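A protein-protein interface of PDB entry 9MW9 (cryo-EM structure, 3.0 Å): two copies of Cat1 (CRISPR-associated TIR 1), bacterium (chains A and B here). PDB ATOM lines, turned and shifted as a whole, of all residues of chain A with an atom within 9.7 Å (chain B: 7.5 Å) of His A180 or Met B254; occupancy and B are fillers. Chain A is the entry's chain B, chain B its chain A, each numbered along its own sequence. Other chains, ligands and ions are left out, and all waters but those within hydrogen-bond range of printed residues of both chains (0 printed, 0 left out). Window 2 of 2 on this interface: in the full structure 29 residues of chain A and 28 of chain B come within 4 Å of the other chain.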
ATOM      1  N   GLY A  50       7.358 -14.197 -11.571  1.00  0.00           N
ATOM      2  CA  GLY A  50       8.040 -13.820 -12.800  1.00  0.00           C
ATOM      3  C   GLY A  50       9.364 -13.135 -12.522  1.00  0.00           C
ATOM      4  O   GLY A  50      10.147 -13.598 -11.693  1.00  0.00           O
ATOM      5  N   ILE A  51       9.608 -12.030 -13.219  1.00  0.00           N
ATOM      6  CA  ILE A  51      10.877 -11.321 -13.154  1.00  0.00           C
ATOM      7  C   ILE A  51      10.680 -10.041 -12.348  1.00  0.00           C
ATOM      8  O   ILE A  51       9.560  -9.671 -11.983  1.00  0.00           O
ATOM      9  CB  ILE A  51      11.424 -11.018 -14.567  1.00  0.00           C
ATOM     10  CG1 ILE A  51      12.946 -10.836 -14.545  1.00  0.00           C
ATOM     11  CG2 ILE A  51      10.735  -9.797 -15.161  1.00  0.00           C
ATOM     12  CD1 ILE A  51      13.702 -12.081 -14.137  1.00  0.00           C
ATOM     13  N   SER A  52      11.797  -9.366 -12.055  1.00  0.00           N
ATOM     14  CA  SER A  52      11.745  -8.106 -11.322  1.00  0.00           C
ATOM     15  C   SER A  52      10.870  -7.074 -12.018  1.00  0.00           C
ATOM     16  O   SER A  52      10.114  -6.363 -11.345  1.00  0.00           O
ATOM     17  CB  SER A  52      13.155  -7.546 -11.134  1.00  0.00           C
ATOM     18  OG  SER A  52      13.743  -7.225 -12.383  1.00  0.00           O
ATOM     19  N   LYS A  53      10.950  -6.975 -13.343  1.00  0.00           N
ATOM     20  CA  LYS A  53       9.983  -6.195 -14.113  1.00  0.00           C
ATOM     21  C   LYS A  53       8.659  -6.963 -14.165  1.00  0.00           C
ATOM     22  O   LYS A  53       8.305  -7.624 -15.141  1.00  0.00           O
ATOM     23  CB  LYS A  53      10.540  -5.889 -15.503  1.00  0.00           C
ATOM     24  CG  LYS A  53       9.549  -5.326 -16.525  1.00  0.00           C
ATOM     25  CD  LYS A  53       8.642  -4.256 -15.938  1.00  0.00           C
ATOM     26  CE  LYS A  53       7.369  -4.136 -16.755  1.00  0.00           C
ATOM     27  NZ  LYS A  53       6.431  -5.255 -16.468  1.00  0.00           N
ATOM     28  N   PRO A 175      19.765  -2.985 -24.797  1.00  0.00           N
ATOM     29  CA  PRO A 175      20.835  -3.869 -24.327  1.00  0.00           C
ATOM     30  C   PRO A 175      20.910  -5.119 -25.187  1.00  0.00           C
ATOM     31  O   PRO A 175      19.895  -5.622 -25.674  1.00  0.00           O
ATOM     32  CB  PRO A 175      20.424  -4.192 -22.887  1.00  0.00           C
ATOM     33  CG  PRO A 175      19.543  -3.062 -22.484  1.00  0.00           C
ATOM     34  CD  PRO A 175      18.815  -2.645 -23.725  1.00  0.00           C
ATOM     35  N   VAL A 176      22.133  -5.612 -25.382  1.00  0.00           N
ATOM     36  CA  VAL A 176      22.344  -6.736 -26.287  1.00  0.00           C
ATOM     37  C   VAL A 176      21.642  -7.984 -25.768  1.00  0.00           C
ATOM     38  O   VAL A 176      21.158  -8.808 -26.554  1.00  0.00           O
ATOM     39  CB  VAL A 176      23.854  -6.962 -26.489  1.00  0.00           C
ATOM     40  CG1 VAL A 176      24.107  -8.169 -27.366  1.00  0.00           C
ATOM     41  CG2 VAL A 176      24.495  -5.718 -27.080  1.00  0.00           C
ATOM     42  N   ASP A 177      21.551  -8.134 -24.449  1.00  0.00           N
ATOM     43  CA  ASP A 177      20.863  -9.258 -23.817  1.00  0.00           C
ATOM     44  C   ASP A 177      19.449  -8.885 -23.389  1.00  0.00           C
ATOM     45  O   ASP A 177      18.968  -9.328 -22.343  1.00  0.00           O
ATOM     46  CB  ASP A 177      21.667  -9.770 -22.627  1.00  0.00           C
ATOM     47  CG  ASP A 177      21.906  -8.698 -21.582  1.00  0.00           C
ATOM     48  OD1 ASP A 177      21.674  -7.508 -21.882  1.00  0.00           O
ATOM     49  OD2 ASP A 177      22.325  -9.044 -20.458  1.00  0.00           O
ATOM     50  N   PHE A 178      18.769  -8.058 -24.187  1.00  0.00           N
ATOM     51  CA  PHE A 178      17.435  -7.593 -23.817  1.00  0.00           C
ATOM     52  C   PHE A 178      16.440  -8.743 -23.737  1.00  0.00           C
ATOM     53  O   PHE A 178      15.598  -8.781 -22.832  1.00  0.00           O
ATOM     54  CB  PHE A 178      16.955  -6.543 -24.818  1.00  0.00           C
ATOM     55  CG  PHE A 178      15.529  -6.129 -24.620  1.00  0.00           C
ATOM     56  CD1 PHE A 178      15.097  -5.653 -23.396  1.00  0.00           C
ATOM     57  CD2 PHE A 178      14.620  -6.218 -25.659  1.00  0.00           C
ATOM     58  CE1 PHE A 178      13.784  -5.273 -23.211  1.00  0.00           C
ATOM     59  CE2 PHE A 178      13.307  -5.838 -25.481  1.00  0.00           C
ATOM     60  CZ  PHE A 178      12.888  -5.367 -24.255  1.00  0.00           C
ATOM     61  N   LEU A 179      16.517  -9.690 -24.675  1.00  0.00           N
ATOM     62  CA  LEU A 179      15.549 -10.781 -24.721  1.00  0.00           C
ATOM     63  C   LEU A 179      15.605 -11.665 -23.483  1.00  0.00           C
ATOM     64  O   LEU A 179      14.631 -12.369 -23.196  1.00  0.00           O
ATOM     65  CB  LEU A 179      15.776 -11.630 -25.971  1.00  0.00           C
ATOM     66  CG  LEU A 179      15.521 -10.941 -27.310  1.00  0.00           C
ATOM     67  CD1 LEU A 179      15.731 -11.911 -28.457  1.00  0.00           C
ATOM     68  CD2 LEU A 179      14.120 -10.359 -27.348  1.00  0.00           C
ATOM     69  N   HIS A 180      16.719 -11.649 -22.748  1.00  0.00           N
ATOM     70  CA  HIS A 180      16.833 -12.483 -21.557  1.00  0.00           C
ATOM     71  C   HIS A 180      15.815 -12.084 -20.497  1.00  0.00           C
ATOM     72  O   HIS A 180      15.219 -12.946 -19.841  1.00  0.00           O
ATOM     73  CB  HIS A 180      18.250 -12.400 -20.993  1.00  0.00           C
ATOM     74  CG  HIS A 180      18.743 -13.686 -20.407  1.00  0.00           C
ATOM     75  ND1 HIS A 180      18.429 -14.088 -19.127  1.00  0.00           N
ATOM     76  CD2 HIS A 180      19.527 -14.660 -20.926  1.00  0.00           C
ATOM     77  CE1 HIS A 180      18.998 -15.255 -18.882  1.00  0.00           C
ATOM     78  NE2 HIS A 180      19.671 -15.624 -19.958  1.00  0.00           N
ATOM     79  N   HIS A 181      15.602 -10.783 -20.312  1.00  0.00           N
ATOM     80  CA  HIS A 181      14.741 -10.276 -19.253  1.00  0.00           C
ATOM     81  C   HIS A 181      13.427  -9.709 -19.773  1.00  0.00           C
ATOM     82  O   HIS A 181      12.740  -8.995 -19.037  1.00  0.00           O
ATOM     83  CB  HIS A 181      15.482  -9.213 -18.439  1.00  0.00           C
ATOM     84  CG  HIS A 181      16.596  -9.760 -17.603  1.00  0.00           C
ATOM     85  ND1 HIS A 181      17.499 -10.687 -18.079  1.00  0.00           N
ATOM     86  CD2 HIS A 181      16.952  -9.513 -16.320  1.00  0.00           C
ATOM     87  CE1 HIS A 181      18.364 -10.986 -17.126  1.00  0.00           C
ATOM     88  NE2 HIS A 181      18.055 -10.287 -16.049  1.00  0.00           N
ATOM     89  N   TRP A 182      13.061 -10.005 -21.016  1.00  0.00           N
ATOM     90  CA  TRP A 182      11.813  -9.519 -21.589  1.00  0.00           C
ATOM     91  C   TRP A 182      10.722 -10.563 -21.380  1.00  0.00           C
ATOM     92  O   TRP A 182      10.824 -11.685 -21.887  1.00  0.00           O
ATOM     93  CB  TRP A 182      11.985  -9.211 -23.075  1.00  0.00           C
ATOM     94  CG  TRP A 182      10.928  -8.306 -23.614  1.00  0.00           C
ATOM     95  CD1 TRP A 182      10.112  -7.482 -22.898  1.00  0.00           C
ATOM     96  CD2 TRP A 182      10.570  -8.129 -24.988  1.00  0.00           C
ATOM     97  NE1 TRP A 182       9.268  -6.802 -23.740  1.00  0.00           N
ATOM     98  CE2 TRP A 182       9.529  -7.183 -25.030  1.00  0.00           C
ATOM     99  CE3 TRP A 182      11.028  -8.680 -26.188  1.00  0.00           C
ATOM    100  CZ2 TRP A 182       8.940  -6.775 -26.222  1.00  0.00           C
ATOM    101  CZ3 TRP A 182      10.441  -8.274 -27.370  1.00  0.00           C
ATOM    102  CH2 TRP A 182       9.409  -7.332 -27.379  1.00  0.00           C
ATOM    103  N   ASP A 183       9.685 -10.193 -20.633  1.00  0.00           N
ATOM    104  CA  ASP A 183       8.576 -11.100 -20.343  1.00  0.00           C
ATOM    105  C   ASP A 183       7.412 -10.820 -21.294  1.00  0.00           C
ATOM    106  O   ASP A 183       6.355 -10.315 -20.914  1.00  0.00           O
ATOM    107  CB  ASP A 183       8.155 -10.973 -18.883  1.00  0.00           C
ATOM    108  CG  ASP A 183       7.939  -9.532 -18.461  1.00  0.00           C
ATOM    109  OD1 ASP A 183       8.105  -8.629 -19.307  1.00  0.00           O
ATOM    110  OD2 ASP A 183       7.594  -9.305 -17.283  1.00  0.00           O
ATOM    111  N   LEU A 184       7.629 -11.164 -22.561  1.00  0.00           N
ATOM    112  CA  LEU A 184       6.611 -11.014 -23.597  1.00  0.00           C
ATOM    113  C   LEU A 184       6.634 -12.258 -24.472  1.00  0.00           C
ATOM    114  O   LEU A 184       7.510 -12.402 -25.330  1.00  0.00           O
ATOM    115  CB  LEU A 184       6.846  -9.751 -24.426  1.00  0.00           C
ATOM    116  CG  LEU A 184       5.736  -9.346 -25.399  1.00  0.00           C
ATOM    117  CD1 LEU A 184       5.609  -7.835 -25.447  1.00  0.00           C
ATOM    118  CD2 LEU A 184       5.997  -9.895 -26.793  1.00  0.00           C
ATOM    119  N   LYS A 185       5.675 -13.153 -24.256  1.00  0.00           N
ATOM    120  CA  LYS A 185       5.535 -14.377 -25.040  1.00  0.00           C
ATOM    121  C   LYS A 185       4.386 -14.158 -26.017  1.00  0.00           C
ATOM    122  O   LYS A 185       3.221 -14.089 -25.616  1.00  0.00           O
ATOM    123  CB  LYS A 185       5.293 -15.608 -24.158  1.00  0.00           C
ATOM    124  CG  LYS A 185       5.914 -15.681 -22.730  1.00  0.00           C
ATOM    125  CD  LYS A 185       7.242 -14.945 -22.476  1.00  0.00           C
ATOM    126  CE  LYS A 185       8.348 -15.362 -23.444  1.00  0.00           C
ATOM    127  NZ  LYS A 185       9.616 -14.622 -23.198  1.00  0.00           N
ATOM    128  N   TRP A 215      17.770  -9.516 -34.938  1.00  0.00           N
ATOM    129  CA  TRP A 215      17.441 -10.547 -33.961  1.00  0.00           C
ATOM    130  C   TRP A 215      16.108 -10.268 -33.282  1.00  0.00           C
ATOM    131  O   TRP A 215      15.417 -11.206 -32.869  1.00  0.00           O
ATOM    132  CB  TRP A 215      18.558 -10.690 -32.925  1.00  0.00           C
ATOM    133  CG  TRP A 215      18.987  -9.415 -32.272  1.00  0.00           C
ATOM    134  CD1 TRP A 215      20.054  -8.640 -32.616  1.00  0.00           C
ATOM    135  CD2 TRP A 215      18.379  -8.780 -31.140  1.00  0.00           C
ATOM    136  NE1 TRP A 215      20.141  -7.555 -31.778  1.00  0.00           N
ATOM    137  CE2 TRP A 215      19.124  -7.619 -30.863  1.00  0.00           C
ATOM    138  CE3 TRP A 215      17.274  -9.078 -30.338  1.00  0.00           C
ATOM    139  CZ2 TRP A 215      18.800  -6.755 -29.821  1.00  0.00           C
ATOM    140  CZ3 TRP A 215      16.953  -8.219 -29.305  1.00  0.00           C
ATOM    141  CH2 TRP A 215      17.714  -7.072 -29.055  1.00  0.00           C
ATOM    142  N   PHE A 219      13.100 -12.925 -33.473  1.00  0.00           N
ATOM    143  CA  PHE A 219      12.463 -13.372 -32.240  1.00  0.00           C
ATOM    144  C   PHE A 219      10.944 -13.302 -32.340  1.00  0.00           C
ATOM    145  O   PHE A 219      10.241 -14.160 -31.795  1.00  0.00           O
ATOM    146  CB  PHE A 219      12.958 -12.536 -31.062  1.00  0.00           C
ATOM    147  CG  PHE A 219      12.203 -12.775 -29.789  1.00  0.00           C
ATOM    148  CD1 PHE A 219      12.402 -13.932 -29.057  1.00  0.00           C
ATOM    149  CD2 PHE A 219      11.293 -11.842 -29.322  1.00  0.00           C
ATOM    150  CE1 PHE A 219      11.709 -14.154 -27.884  1.00  0.00           C
ATOM    151  CE2 PHE A 219      10.596 -12.060 -28.151  1.00  0.00           C
ATOM    152  CZ  PHE A 219      10.805 -13.218 -27.431  1.00  0.00           C
ATOM    153  N   THR B 160      30.008 -23.436 -25.856  1.00  0.00           N
ATOM    154  CA  THR B 160      28.717 -23.853 -26.386  1.00  0.00           C
ATOM    155  C   THR B 160      28.901 -24.307 -27.828  1.00  0.00           C
ATOM    156  O   THR B 160      29.422 -23.554 -28.657  1.00  0.00           O
ATOM    157  CB  THR B 160      27.696 -22.718 -26.303  1.00  0.00           C
ATOM    158  OG1 THR B 160      27.191 -22.626 -24.966  1.00  0.00           O
ATOM    159  CG2 THR B 160      26.538 -22.969 -27.254  1.00  0.00           C
ATOM    160  N   PHE B 231      20.552 -19.045 -33.437  1.00  0.00           N
ATOM    161  CA  PHE B 231      21.342 -17.891 -33.037  1.00  0.00           C
ATOM    162  C   PHE B 231      21.448 -16.932 -34.213  1.00  0.00           C
ATOM    163  O   PHE B 231      21.563 -17.360 -35.366  1.00  0.00           O
ATOM    164  CB  PHE B 231      22.739 -18.305 -32.574  1.00  0.00           C
ATOM    165  CG  PHE B 231      22.809 -18.694 -31.128  1.00  0.00           C
ATOM    166  CD1 PHE B 231      22.555 -19.996 -30.734  1.00  0.00           C
ATOM    167  CD2 PHE B 231      23.138 -17.761 -30.162  1.00  0.00           C
ATOM    168  CE1 PHE B 231      22.623 -20.357 -29.405  1.00  0.00           C
ATOM    169  CE2 PHE B 231      23.208 -18.117 -28.831  1.00  0.00           C
ATOM    170  CZ  PHE B 231      22.950 -19.415 -28.452  1.00  0.00           C
ATOM    171  N   VAL B 232      21.407 -15.636 -33.922  1.00  0.00           N
ATOM    172  CA  VAL B 232      21.482 -14.592 -34.938  1.00  0.00           C
ATOM    173  C   VAL B 232      22.662 -13.690 -34.608  1.00  0.00           C
ATOM    174  O   VAL B 232      22.834 -13.284 -33.453  1.00  0.00           O
ATOM    175  CB  VAL B 232      20.177 -13.779 -35.019  1.00  0.00           C
ATOM    176  CG1 VAL B 232      20.258 -12.763 -36.138  1.00  0.00           C
ATOM    177  CG2 VAL B 232      18.991 -14.703 -35.225  1.00  0.00           C
ATOM    178  N   GLU B 239      28.320 -10.236 -31.658  1.00  0.00           N
ATOM    179  CA  GLU B 239      28.140 -11.538 -31.031  1.00  0.00           C
ATOM    180  C   GLU B 239      26.912 -12.205 -31.635  1.00  0.00           C
ATOM    181  O   GLU B 239      26.202 -11.624 -32.459  1.00  0.00           O
ATOM    182  CB  GLU B 239      27.990 -11.464 -29.504  1.00  0.00           C
ATOM    183  CG  GLU B 239      28.959 -10.567 -28.762  1.00  0.00           C
ATOM    184  CD  GLU B 239      28.376  -9.212 -28.446  1.00  0.00           C
ATOM    185  OE1 GLU B 239      27.183  -9.150 -28.085  1.00  0.00           O
ATOM    186  OE2 GLU B 239      29.119  -8.216 -28.521  1.00  0.00           O
ATOM    187  N   TYR B 240      26.667 -13.441 -31.213  1.00  0.00           N
ATOM    188  CA  TYR B 240      25.487 -14.192 -31.614  1.00  0.00           C
ATOM    189  C   TYR B 240      24.404 -14.029 -30.558  1.00  0.00           C
ATOM    190  O   TYR B 240      24.682 -14.070 -29.357  1.00  0.00           O
ATOM    191  CB  TYR B 240      25.820 -15.673 -31.799  1.00  0.00           C
ATOM    192  CG  TYR B 240      26.715 -15.955 -32.982  1.00  0.00           C
ATOM    193  CD1 TYR B 240      26.193 -16.071 -34.261  1.00  0.00           C
ATOM    194  CD2 TYR B 240      28.084 -16.105 -32.818  1.00  0.00           C
ATOM    195  CE1 TYR B 240      27.009 -16.329 -35.343  1.00  0.00           C
ATOM    196  CE2 TYR B 240      28.907 -16.362 -33.893  1.00  0.00           C
ATOM    197  CZ  TYR B 240      28.364 -16.474 -35.154  1.00  0.00           C
ATOM    198  OH  TYR B 240      29.182 -16.730 -36.230  1.00  0.00           O
ATOM    199  N   ILE B 241      23.168 -13.843 -31.011  1.00  0.00           N
ATOM    200  CA  ILE B 241      22.028 -13.609 -30.132  1.00  0.00           C
ATOM    201  C   ILE B 241      21.078 -14.789 -30.251  1.00  0.00           C
ATOM    202  O   ILE B 241      20.689 -15.172 -31.361  1.00  0.00           O
ATOM    203  CB  ILE B 241      21.311 -12.294 -30.476  1.00  0.00           C
ATOM    204  CG1 ILE B 241      22.323 -11.173 -30.719  1.00  0.00           C
ATOM    205  CG2 ILE B 241      20.357 -11.907 -29.360  1.00  0.00           C
ATOM    206  CD1 ILE B 241      23.254 -10.930 -29.560  1.00  0.00           C
ATOM    207  N   CYS B 242      20.703 -15.361 -29.111  1.00  0.00           N
ATOM    208  CA  CYS B 242      19.765 -16.474 -29.076  1.00  0.00           C
ATOM    209  C   CYS B 242      18.339 -15.943 -29.124  1.00  0.00           C
ATOM    210  O   CYS B 242      17.954 -15.106 -28.302  1.00  0.00           O
ATOM    211  CB  CYS B 242      19.972 -17.318 -27.819  1.00  0.00           C
ATOM    212  SG  CYS B 242      18.942 -18.796 -27.737  1.00  0.00           S
ATOM    213  N   VAL B 243      17.562 -16.430 -30.088  1.00  0.00           N
ATOM    214  CA  VAL B 243      16.172 -16.031 -30.223  1.00  0.00           C
ATOM    215  C   VAL B 243      15.205 -17.171 -29.915  1.00  0.00           C
ATOM    216  O   VAL B 243      14.124 -16.916 -29.371  1.00  0.00           O
ATOM    217  CB  VAL B 243      15.904 -15.452 -31.626  1.00  0.00           C
ATOM    218  CG1 VAL B 243      16.559 -14.092 -31.763  1.00  0.00           C
ATOM    219  CG2 VAL B 243      16.419 -16.394 -32.693  1.00  0.00           C
ATOM    220  N   SER B 245      14.797 -21.043 -28.005  1.00  0.00           N
ATOM    221  CA  SER B 245      15.394 -21.927 -27.008  1.00  0.00           C
ATOM    222  C   SER B 245      14.679 -23.271 -27.063  1.00  0.00           C
ATOM    223  O   SER B 245      13.626 -23.449 -26.444  1.00  0.00           O
ATOM    224  CB  SER B 245      15.310 -21.316 -25.614  1.00  0.00           C
ATOM    225  OG  SER B 245      16.241 -21.924 -24.737  1.00  0.00           O
ATOM    226  N   GLY B 249      19.446 -25.533 -20.929  1.00  0.00           N
ATOM    227  CA  GLY B 249      20.659 -24.840 -20.555  1.00  0.00           C
ATOM    228  C   GLY B 249      20.851 -23.479 -21.185  1.00  0.00           C
ATOM    229  O   GLY B 249      21.767 -22.753 -20.778  1.00  0.00           O
ATOM    230  N   LEU B 250      20.027 -23.104 -22.159  1.00  0.00           N
ATOM    231  CA  LEU B 250      20.114 -21.795 -22.786  1.00  0.00           C
ATOM    232  C   LEU B 250      18.719 -21.209 -22.952  1.00  0.00           C
ATOM    233  O   LEU B 250      17.729 -21.937 -23.062  1.00  0.00           O
ATOM    234  CB  LEU B 250      20.842 -21.863 -24.140  1.00  0.00           C
ATOM    235  CG  LEU B 250      20.540 -23.006 -25.112  1.00  0.00           C
ATOM    236  CD1 LEU B 250      19.232 -22.785 -25.859  1.00  0.00           C
ATOM    237  CD2 LEU B 250      21.693 -23.183 -26.086  1.00  0.00           C
ATOM    238  N   ALA B 251      18.655 -19.882 -22.965  1.00  0.00           N
ATOM    239  CA  ALA B 251      17.417 -19.129 -23.048  1.00  0.00           C
ATOM    240  C   ALA B 251      17.544 -18.055 -24.117  1.00  0.00           C
ATOM    241  O   ALA B 251      18.659 -17.642 -24.453  1.00  0.00           O
ATOM    242  CB  ALA B 251      17.078 -18.482 -21.697  1.00  0.00           C
ATOM    243  N   PRO B 252      16.422 -17.586 -24.678  1.00  0.00           N
ATOM    244  CA  PRO B 252      16.509 -16.541 -25.706  1.00  0.00           C
ATOM    245  C   PRO B 252      16.997 -15.223 -25.132  1.00  0.00           C
ATOM    246  O   PRO B 252      16.292 -14.577 -24.352  1.00  0.00           O
ATOM    247  CB  PRO B 252      15.069 -16.427 -26.227  1.00  0.00           C
ATOM    248  CG  PRO B 252      14.350 -17.626 -25.702  1.00  0.00           C
ATOM    249  CD  PRO B 252      15.031 -17.997 -24.432  1.00  0.00           C
ATOM    250  N   GLY B 253      18.206 -14.818 -25.510  1.00  0.00           N
ATOM    251  CA  GLY B 253      18.763 -13.574 -25.021  1.00  0.00           C
ATOM    252  C   GLY B 253      20.221 -13.680 -24.631  1.00  0.00           C
ATOM    253  O   GLY B 253      20.894 -12.662 -24.443  1.00  0.00           O
ATOM    254  N   MET B 254      20.725 -14.904 -24.501  1.00  0.00           N
ATOM    255  CA  MET B 254      22.126 -15.088 -24.162  1.00  0.00           C
ATOM    256  C   MET B 254      23.013 -14.705 -25.342  1.00  0.00           C
ATOM    257  O   MET B 254      22.585 -14.688 -26.500  1.00  0.00           O
ATOM    258  CB  MET B 254      22.396 -16.530 -23.733  1.00  0.00           C
ATOM    259  CG  MET B 254      22.764 -17.467 -24.867  1.00  0.00           C
ATOM    260  SD  MET B 254      23.707 -18.885 -24.280  1.00  0.00           S
ATOM    261  CE  MET B 254      22.877 -19.220 -22.729  1.00  0.00           C
ATOM    262  N   VAL B 255      24.266 -14.387 -25.034  1.00  0.00           N
ATOM    263  CA  VAL B 255      25.204 -13.840 -26.004  1.00  0.00           C
ATOM    264  C   VAL B 255      26.459 -14.697 -26.025  1.00  0.00           C
ATOM    265  O   VAL B 255      26.896 -15.202 -24.985  1.00  0.00           O
ATOM    266  CB  VAL B 255      25.551 -12.374 -25.681  1.00  0.00           C
ATOM    267  CG1 VAL B 255      24.417 -11.469 -26.102  1.00  0.00           C
ATOM    268  CG2 VAL B 255      25.839 -12.216 -24.199  1.00  0.00           C
ATOM    269  N   LEU B 256      27.032 -14.863 -27.212  1.00  0.00           N
ATOM    270  CA  LEU B 256      28.272 -15.609 -27.407  1.00  0.00           C
ATOM    271  C   LEU B 256      29.318 -14.631 -27.938  1.00  0.00           C
ATOM    272  O   LEU B 256      29.359 -14.332 -29.132  1.00  0.00           O
ATOM    273  CB  LEU B 256      28.062 -16.780 -28.358  1.00  0.00           C
ATOM    274  CG  LEU B 256      26.982 -17.787 -27.962  1.00  0.00           C
ATOM    275  CD1 LEU B 256      27.039 -19.010 -28.860  1.00  0.00           C
ATOM    276  CD2 LEU B 256      27.129 -18.184 -26.503  1.00  0.00           C
ATOM    277  N   LYS B 257      30.165 -14.137 -27.039  1.00  0.00           N
ATOM    278  CA  LYS B 257      31.185 -13.172 -27.424  1.00  0.00           C
ATOM    279  C   LYS B 257      32.174 -13.800 -28.398  1.00  0.00           C
ATOM    280  O   LYS B 257      32.635 -14.928 -28.203  1.00  0.00           O
ATOM    281  CB  LYS B 257      31.914 -12.651 -26.182  1.00  0.00           C
ATOM    282  CG  LYS B 257      33.073 -11.702 -26.470  1.00  0.00           C
ATOM    283  CD  LYS B 257      34.422 -12.406 -26.386  1.00  0.00           C
ATOM    284  CE  LYS B 257      35.569 -11.408 -26.433  1.00  0.00           C
ATOM    285  NZ  LYS B 257      36.841 -12.044 -26.874  1.00  0.00           N
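O of Cys B242 sits at hydrogen-bond distance from N of Gly B253 (2.8 Å).
N of Ile B241 lies within hydrogen-bond range of O of Val B232.
The backbone NH (N) of Cys B242 lies within hydrogen-bond range of the backbone carbonyl oxygen (O) of Met B254.
SG of Cys B242 is in hydrogen-bond range of O of Ala B251, at 3.5 Å.
The backbone carbonyl oxygen (O) of Leu A179 sits close to the backbone carbonyl oxygen (O) of Pro B252 (3.0 Å).
The backbone carbonyl oxygen (O) of Pro B252 lies within hydrogen-bond range of the backbone NH (N) of His A180, at 3.4 Å.
No position is printed for both chains.
Of the 13 pairs that touch across the chains among the printed residues, none has its exchanged pair printed and touching as well.
Of the 17 printed residues of chain A, 6 touch a printed residue of chain B.
Printed residues of chain A that touch a printed residue of chain B: Val A176, Asp A177, Leu A179, His A180, Trp A215 and Phe A219.
Hydrophobic or aromatic side chains of chain B that line the printed part of chain A: Ile B241, Val B243 and Val B255.
Among the printed residues, 13 pairs touch across the chains.
Among the printed residues, no Asp or Glu carboxylate lies within 4 Å of a Lys or Arg side-chain nitrogen of the other chain.
His A180 touches three residues of chain B.
Met B254 touches just one residue of chain A: His A180.
Ile B241 touches just these residues of chain A: Val A176 and Trp A215.
Cys B242 touches just one residue of chain A: Leu A179 (3.9 Å).
No residue of chain A comes within 4 Å of Ala B251.
Gly B253 touches three residues of chain A.
Val B255 touches just one residue of chain A: Val A176.
Of the printed residues of chain B, Val A176 touches Glu B239, Ile B241 and Val B255.
Of the printed residues of chain B, Trp A215 touches Ile B241 and Val B243.
Of the printed residues of chain A, Val B243 touches Trp A215 (3.3 Å) and Phe A219 (3.5 Å).
Of the printed residues of chain B, Phe A219 touches Val B243.
Of the printed residues of chain B, Leu A179 touches Cys B242, Pro B252 and Gly B253.
Leu A184 touches none of the printed residues of chain B.
His A181 touches none of the printed residues of chain B.
The nearest residue of chain A that does not touch Met B254 is Asp A177 (5.5 Å).
The nearest printed residue of chain B that does not touch Asp A177 is Val B255 (4.7 Å).
Val A176 touches Glu B239.
Val A176 touches Val B255 (CG1 to CG1, 3.5 Å).
Asp A177 touches Gly B253.
CD1 of Leu A179 touches O of Cys B242, 3.9 Å away.
CB of Leu A179 touches CA of Gly B253, at 3.7 Å.
His A180 touches Gly B253.
CD2 of His A180 touches N of Met B254 (3.8 Å).
Trp A215 touches Ile B241 (CD1 to CG1, 3.9 Å).
CG1 of Val B243 touches O of Trp A215, 3.3 Å away.
CD1 of Phe A219 touches O of Val B243, 3.5 Å away.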
